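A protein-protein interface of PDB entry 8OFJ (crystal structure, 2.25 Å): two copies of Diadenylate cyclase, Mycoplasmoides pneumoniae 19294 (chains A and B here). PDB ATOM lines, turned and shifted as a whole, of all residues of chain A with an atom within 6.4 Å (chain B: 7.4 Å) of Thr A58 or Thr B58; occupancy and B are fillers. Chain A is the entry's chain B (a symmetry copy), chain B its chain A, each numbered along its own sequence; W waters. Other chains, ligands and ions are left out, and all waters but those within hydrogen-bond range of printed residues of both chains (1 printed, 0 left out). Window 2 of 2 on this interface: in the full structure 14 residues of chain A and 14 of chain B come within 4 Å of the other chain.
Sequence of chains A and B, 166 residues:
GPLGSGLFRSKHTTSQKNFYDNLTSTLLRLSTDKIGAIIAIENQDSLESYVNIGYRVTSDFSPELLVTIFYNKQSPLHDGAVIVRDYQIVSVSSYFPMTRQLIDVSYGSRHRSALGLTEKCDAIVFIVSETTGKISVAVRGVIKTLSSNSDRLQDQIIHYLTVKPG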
ATOM      1  N   ARG A  56     -26.507 -11.045  20.753  1.00  0.00           N
ATOM      2  CA  ARG A  56     -27.027 -11.478  22.048  1.00  0.00           C
ATOM      3  C   ARG A  56     -25.858 -11.712  23.000  1.00  0.00           C
ATOM      4  O   ARG A  56     -25.060 -12.611  22.775  1.00  0.00           O
ATOM      5  CB  ARG A  56     -27.864 -12.759  21.958  1.00  0.00           C
ATOM      6  CG  ARG A  56     -29.084 -12.674  21.049  1.00  0.00           C
ATOM      7  N   VAL A  57     -25.779 -10.886  24.050  1.00  0.00           N
ATOM      8  CA  VAL A  57     -24.726 -10.942  25.050  1.00  0.00           C
ATOM      9  C   VAL A  57     -25.366 -10.812  26.422  1.00  0.00           C
ATOM     10  O   VAL A  57     -25.802  -9.730  26.772  1.00  0.00           O
ATOM     11  CB  VAL A  57     -23.693  -9.820  24.857  1.00  0.00           C
ATOM     12  CG1 VAL A  57     -22.675  -9.774  25.995  1.00  0.00           C
ATOM     13  CG2 VAL A  57     -22.985  -9.944  23.516  1.00  0.00           C
ATOM     14  N   THR A  58     -25.383 -11.893  27.199  1.00  0.00           N
ATOM     15  CA  THR A  58     -25.937 -11.850  28.542  1.00  0.00           C
ATOM     16  C   THR A  58     -24.814 -11.580  29.545  1.00  0.00           C
ATOM     17  O   THR A  58     -23.773 -12.222  29.495  1.00  0.00           O
ATOM     18  CB  THR A  58     -26.711 -13.131  28.862  1.00  0.00           C
ATOM     19  OG1 THR A  58     -27.473 -13.438  27.694  1.00  0.00           O
ATOM     20  CG2 THR A  58     -27.622 -12.979  30.058  1.00  0.00           C
ATOM     21  N   SER A  59     -25.027 -10.608  30.440  1.00  0.00           N
ATOM     22  CA  SER A  59     -24.018 -10.244  31.422  1.00  0.00           C
ATOM     23  C   SER A  59     -24.609  -9.256  32.417  1.00  0.00           C
ATOM     24  O   SER A  59     -25.589  -8.573  32.109  1.00  0.00           O
ATOM     25  CB  SER A  59     -22.783  -9.669  30.761  1.00  0.00           C
ATOM     26  OG  SER A  59     -21.881  -9.124  31.720  1.00  0.00           O
ATOM     27  N   ASP A  60     -23.988  -9.196  33.599  1.00  0.00           N
ATOM     28  CA  ASP A  60     -24.228  -8.140  34.567  1.00  0.00           C
ATOM     29  C   ASP A  60     -23.926  -6.788  33.928  1.00  0.00           C
ATOM     30  O   ASP A  60     -23.133  -6.700  32.985  1.00  0.00           O
ATOM     31  CB  ASP A  60     -23.379  -8.333  35.827  1.00  0.00           C
ATOM     32  CG  ASP A  60     -23.879  -9.452  36.727  1.00  0.00           C
ATOM     33  OD1 ASP A  60     -25.052  -9.873  36.557  1.00  0.00           O
ATOM     34  OD2 ASP A  60     -23.091  -9.915  37.578  1.00  0.00           O
ATOM     35  N   GLN A  88     -29.747  -6.454  33.558  1.00  0.00           N
ATOM     36  CA  GLN A  88     -28.731  -7.229  32.866  1.00  0.00           C
ATOM     37  C   GLN A  88     -28.673  -6.769  31.416  1.00  0.00           C
ATOM     38  O   GLN A  88     -29.702  -6.459  30.827  1.00  0.00           O
ATOM     39  CB  GLN A  88     -29.067  -8.725  32.812  1.00  0.00           C
ATOM     40  CG  GLN A  88     -29.523  -9.328  34.134  1.00  0.00           C
ATOM     41  CD  GLN A  88     -28.408  -9.350  35.141  1.00  0.00           C
ATOM     42  OE1 GLN A  88     -28.536  -8.805  36.233  1.00  0.00           O
ATOM     43  NE2 GLN A  88     -27.311  -9.995  34.775  1.00  0.00           N
ATOM     44  N   ILE A  89     -27.474  -6.806  30.846  1.00  0.00           N
ATOM     45  CA  ILE A  89     -27.285  -6.643  29.418  1.00  0.00           C
ATOM     46  C   ILE A  89     -27.796  -7.889  28.702  1.00  0.00           C
ATOM     47  O   ILE A  89     -27.443  -9.005  29.087  1.00  0.00           O
ATOM     48  CB  ILE A  89     -25.800  -6.428  29.104  1.00  0.00           C
ATOM     49  CG1 ILE A  89     -25.274  -5.144  29.751  1.00  0.00           C
ATOM     50  CG2 ILE A  89     -25.571  -6.454  27.603  1.00  0.00           C
ATOM     51  CD1 ILE A  89     -23.756  -5.044  29.774  1.00  0.00           C
ATOM     52  N   VAL A  90     -28.567  -7.695  27.621  1.00  0.00           N
ATOM     53  CA  VAL A  90     -29.045  -8.830  26.855  1.00  0.00           C
ATOM     54  C   VAL A  90     -28.638  -8.718  25.383  1.00  0.00           C
ATOM     55  O   VAL A  90     -28.729  -9.697  24.655  1.00  0.00           O
ATOM     56  CB  VAL A  90     -30.556  -9.014  27.053  1.00  0.00           C
ATOM     57  CG1 VAL A  90     -30.845  -9.610  28.414  1.00  0.00           C
ATOM     58  CG2 VAL A  90     -31.327  -7.718  26.863  1.00  0.00           C
ATOM     59  N   SER A  91     -28.204  -7.548  24.918  1.00  0.00           N
ATOM     60  CA  SER A  91     -27.768  -7.424  23.539  1.00  0.00           C
ATOM     61  C   SER A  91     -26.921  -6.182  23.393  1.00  0.00           C
ATOM     62  O   SER A  91     -27.051  -5.256  24.192  1.00  0.00           O
ATOM     63  CB  SER A  91     -28.915  -7.389  22.544  1.00  0.00           C
ATOM     64  OG  SER A  91     -29.421  -6.070  22.382  1.00  0.00           O
ATOM     65  N   TYR B  55     -15.904 -13.886  35.162  1.00  0.00           N
ATOM     66  CA  TYR B  55     -17.108 -13.102  34.990  1.00  0.00           C
ATOM     67  C   TYR B  55     -17.967 -13.765  33.923  1.00  0.00           C
ATOM     68  O   TYR B  55     -17.529 -13.921  32.786  1.00  0.00           O
ATOM     69  CB  TYR B  55     -16.741 -11.658  34.650  1.00  0.00           C
ATOM     70  CG  TYR B  55     -16.091 -10.922  35.796  1.00  0.00           C
ATOM     71  CD1 TYR B  55     -16.749 -10.794  37.012  1.00  0.00           C
ATOM     72  CD2 TYR B  55     -14.827 -10.350  35.674  1.00  0.00           C
ATOM     73  CE1 TYR B  55     -16.172 -10.126  38.080  1.00  0.00           C
ATOM     74  CE2 TYR B  55     -14.236  -9.674  36.734  1.00  0.00           C
ATOM     75  CZ  TYR B  55     -14.915  -9.563  37.939  1.00  0.00           C
ATOM     76  OH  TYR B  55     -14.391  -8.894  39.026  1.00  0.00           O
ATOM     77  N   ARG B  56     -19.183 -14.151  34.324  1.00  0.00           N
ATOM     78  CA  ARG B  56     -20.133 -14.803  33.444  1.00  0.00           C
ATOM     79  C   ARG B  56     -20.572 -13.836  32.360  1.00  0.00           C
ATOM     80  O   ARG B  56     -21.214 -12.822  32.627  1.00  0.00           O
ATOM     81  CB  ARG B  56     -21.359 -15.303  34.213  1.00  0.00           C
ATOM     82  CG  ARG B  56     -21.089 -16.528  35.073  1.00  0.00           C
ATOM     83  CD  ARG B  56     -22.164 -16.721  36.133  1.00  0.00           C
ATOM     84  NE  ARG B  56     -21.639 -17.204  37.405  1.00  0.00           N
ATOM     85  CZ  ARG B  56     -20.782 -16.539  38.196  1.00  0.00           C
ATOM     86  NH1 ARG B  56     -20.203 -15.415  37.801  1.00  0.00           N
ATOM     87  NH2 ARG B  56     -20.490 -17.017  39.396  1.00  0.00           N
ATOM     88  N   VAL B  57     -20.220 -14.181  31.128  1.00  0.00           N
ATOM     89  CA  VAL B  57     -20.726 -13.492  29.964  1.00  0.00           C
ATOM     90  C   VAL B  57     -21.110 -14.577  28.966  1.00  0.00           C
ATOM     91  O   VAL B  57     -20.285 -15.431  28.652  1.00  0.00           O
ATOM     92  CB  VAL B  57     -19.687 -12.502  29.407  1.00  0.00           C
ATOM     93  CG1 VAL B  57     -18.454 -13.202  28.882  1.00  0.00           C
ATOM     94  CG2 VAL B  57     -20.266 -11.626  28.321  1.00  0.00           C
ATOM     95  N   THR B  58     -22.369 -14.561  28.512  1.00  0.00           N
ATOM     96  CA  THR B  58     -22.842 -15.526  27.533  1.00  0.00           C
ATOM     97  C   THR B  58     -23.047 -14.849  26.181  1.00  0.00           C
ATOM     98  O   THR B  58     -23.722 -13.828  26.108  1.00  0.00           O
ATOM     99  CB  THR B  58     -24.157 -16.179  27.975  1.00  0.00           C
ATOM    100  OG1 THR B  58     -23.933 -16.731  29.267  1.00  0.00           O
ATOM    101  CG2 THR B  58     -24.639 -17.260  27.034  1.00  0.00           C
ATOM    102  N   SER B  59     -22.486 -15.456  25.130  1.00  0.00           N
ATOM    103  CA  SER B  59     -22.610 -14.955  23.774  1.00  0.00           C
ATOM    104  C   SER B  59     -22.078 -15.974  22.773  1.00  0.00           C
ATOM    105  O   SER B  59     -21.346 -16.902  23.119  1.00  0.00           O
ATOM    106  CB  SER B  59     -21.878 -13.637  23.633  1.00  0.00           C
ATOM    107  OG  SER B  59     -21.959 -13.130  22.311  1.00  0.00           O
ATOM    108  N   ASP B  60     -22.434 -15.775  21.509  1.00  0.00           N
ATOM    109  CA  ASP B  60     -21.824 -16.515  20.420  1.00  0.00           C
ATOM    110  C   ASP B  60     -20.346 -16.158  20.369  1.00  0.00           C
ATOM    111  O   ASP B  60     -19.983 -15.036  20.714  1.00  0.00           O
ATOM    112  CB  ASP B  60     -22.479 -16.200  19.073  1.00  0.00           C
ATOM    113  CG  ASP B  60     -23.878 -16.766  18.944  1.00  0.00           C
ATOM    114  OD1 ASP B  60     -24.245 -17.594  19.797  1.00  0.00           O
ATOM    115  OD2 ASP B  60     -24.594 -16.362  18.000  1.00  0.00           O
ATOM    116  N   LEU B  65     -16.700  -9.549  19.452  1.00  0.00           N
ATOM    117  CA  LEU B  65     -16.737  -9.480  20.902  1.00  0.00           C
ATOM    118  C   LEU B  65     -15.339  -9.730  21.463  1.00  0.00           C
ATOM    119  O   LEU B  65     -14.889  -9.003  22.334  1.00  0.00           O
ATOM    120  CB  LEU B  65     -17.771 -10.474  21.437  1.00  0.00           C
ATOM    121  CG  LEU B  65     -17.892 -10.557  22.958  1.00  0.00           C
ATOM    122  CD1 LEU B  65     -18.323  -9.231  23.565  1.00  0.00           C
ATOM    123  CD2 LEU B  65     -18.871 -11.651  23.358  1.00  0.00           C
ATOM    124  N   ARG B  85     -18.188 -23.026  25.747  1.00  0.00           N
ATOM    125  CA  ARG B  85     -19.023 -24.204  25.875  1.00  0.00           C
ATOM    126  C   ARG B  85     -20.045 -24.200  24.735  1.00  0.00           C
ATOM    127  O   ARG B  85     -20.820 -23.253  24.597  1.00  0.00           O
ATOM    128  CB  ARG B  85     -19.733 -24.190  27.234  1.00  0.00           C
ATOM    129  CG  ARG B  85     -20.622 -25.397  27.479  1.00  0.00           C
ATOM    130  CD  ARG B  85     -21.556 -25.194  28.651  1.00  0.00           C
ATOM    131  NE  ARG B  85     -20.803 -25.140  29.888  1.00  0.00           N
ATOM    132  CZ  ARG B  85     -21.022 -24.305  30.892  1.00  0.00           C
ATOM    133  NH1 ARG B  85     -22.101 -23.543  30.909  1.00  0.00           N
ATOM    134  NH2 ARG B  85     -20.163 -24.261  31.901  1.00  0.00           N
ATOM    135  N   GLN B  88     -20.185 -21.351  22.449  1.00  0.00           N
ATOM    136  CA  GLN B  88     -20.519 -20.080  23.063  1.00  0.00           C
ATOM    137  C   GLN B  88     -19.535 -19.746  24.177  1.00  0.00           C
ATOM    138  O   GLN B  88     -19.205 -20.591  25.012  1.00  0.00           O
ATOM    139  CB  GLN B  88     -21.916 -20.098  23.680  1.00  0.00           C
ATOM    140  CG  GLN B  88     -23.044 -20.233  22.669  1.00  0.00           C
ATOM    141  CD  GLN B  88     -24.256 -19.473  23.157  1.00  0.00           C
ATOM    142  OE1 GLN B  88     -24.696 -19.624  24.295  1.00  0.00           O
ATOM    143  NE2 GLN B  88     -24.777 -18.598  22.314  1.00  0.00           N
ATOM    144  N   ILE B  89     -19.133 -18.468  24.209  1.00  0.00           N
ATOM    145  CA  ILE B  89     -18.472 -17.868  25.356  1.00  0.00           C
ATOM    146  C   ILE B  89     -19.406 -17.935  26.561  1.00  0.00           C
ATOM    147  O   ILE B  89     -20.553 -17.509  26.470  1.00  0.00           O
ATOM    148  CB  ILE B  89     -18.064 -16.424  25.030  1.00  0.00           C
ATOM    149  CG1 ILE B  89     -17.119 -16.383  23.828  1.00  0.00           C
ATOM    150  CG2 ILE B  89     -17.448 -15.731  26.234  1.00  0.00           C
ATOM    151  CD1 ILE B  89     -17.291 -15.143  22.979  1.00  0.00           C
ATOM    152  N   VAL B  90     -18.884 -18.440  27.689  1.00  0.00           N
ATOM    153  CA  VAL B  90     -19.634 -18.506  28.930  1.00  0.00           C
ATOM    154  C   VAL B  90     -18.952 -17.725  30.057  1.00  0.00           C
ATOM    155  O   VAL B  90     -19.576 -17.462  31.077  1.00  0.00           O
ATOM    156  CB  VAL B  90     -19.892 -19.969  29.329  1.00  0.00           C
ATOM    157  CG1 VAL B  90     -20.872 -20.625  28.364  1.00  0.00           C
ATOM    158  CG2 VAL B  90     -18.618 -20.781  29.423  1.00  0.00           C
ATOM    159  N   SER B  91     -17.672 -17.363  29.907  1.00  0.00           N
ATOM    160  CA  SER B  91     -17.002 -16.549  30.910  1.00  0.00           C
ATOM    161  C   SER B  91     -15.736 -15.953  30.324  1.00  0.00           C
ATOM    162  O   SER B  91     -15.223 -16.465  29.336  1.00  0.00           O
ATOM    163  CB  SER B  91     -16.658 -17.326  32.181  1.00  0.00           C
ATOM    164  OG  SER B  91     -15.573 -18.220  31.958  1.00  0.00           O
HETATM  165  O   HOH W   1     -22.504 -11.486  34.431  1.00  0.00           O
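The backbone carbonyl oxygen (O) of Ser A59 is in hydrogen-bond range of the side-chain amide nitrogen (NE2) of Gln A88 (3.5 Å). The backbone NH (N) of Val A57 lies within hydrogen-bond range of the backbone carbonyl oxygen (O) of Val A90, 3.2 Å away. The backbone carbonyl oxygen of Val B57 sits at hydrogen-bond distance from the backbone NH of Ser B91 (3.5 Å). O of Ser A59 sits at hydrogen-bond distance from N of Ile A89 (2.9 Å). The backbone carbonyl oxygen (O) of Ser B59 sits at hydrogen-bond distance from the backbone NH (N) of Ile B89, at 2.9 Å. N of Val B57 sits at hydrogen-bond distance from O of Val B90, 3.3 Å away.
Water W1 lies within hydrogen-bond range of O of Arg B56 and N of Asp A60.
Thr A58 touches just these residues of chain B: Val B57 (3.3 Å) and Thr B58 (2.8 Å). Of chain A, only Arg A56, Val A57 and Thr A58 come within 4 Å of Thr B58. Of the printed residues of chain A, Arg B56 touches Ser A59. Of the printed residues of chain B, Arg A56 touches Thr B58 (3.8 Å) and Ser B59 (3.2 Å). Of the printed residues of chain A, Val B57 touches Val A57 (3.8 Å) and Thr A58 (3.3 Å). Ser B91 touches none of the printed residues of chain A. Val B90 touches none of the printed residues of chain A. The nearest residue of chain B that does not touch Thr A58 is Arg B56 (4.1 Å). The nearest residue of chain A that does not touch Thr B58 is Ser A59 (5.1 Å). The nearest printed residue of chain A that does not touch Arg B56 is Thr A58 (4.1 Å).
The backbone carbonyl oxygen (O) of Thr B58 is in hydrogen-bond range of the backbone NH (N) of Thr A58, 2.8 Å away. The side-chain hydroxyl (OG) of Ser B59 is in hydrogen-bond range of the backbone carbonyl oxygen (O) of Arg A56.
Among the printed residues, merely in contact across the chains: Val A57 with Thr B58, Thr A58 with Val B57, Val A57 with Ser B59, Arg A56 with Thr B58, Val A57 with Val B57 and Ser A59 with Arg B56.
Arg A56 touches Thr B58, but with the chains exchanged Thr A58 does not touch Arg B56 (4.1 Å). Arg A56 touches Ser B59, and with the chains exchanged Ser A59 touches Arg B56. Val A57 touches Thr B58, and with the chains exchanged Thr A58 touches Val B57. Thr A58 touches its own counterpart, Thr B58. 9 positions are printed for both chains. Of the 8 pairs that touch across the chains among the printed residues, 6 have their exchanged pair printed and touching as well.
Of the 12 printed residues of chain B, 4 touch a printed residue of chain A. Hydrophobic or aromatic side chains of chain B that line the printed part of chain A: Val B57. Printed residues of chain A that touch a printed residue of chain B: Arg A56, Val A57, Thr A58 and Ser A59. Among the printed residues, 8 pairs touch across the chains.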
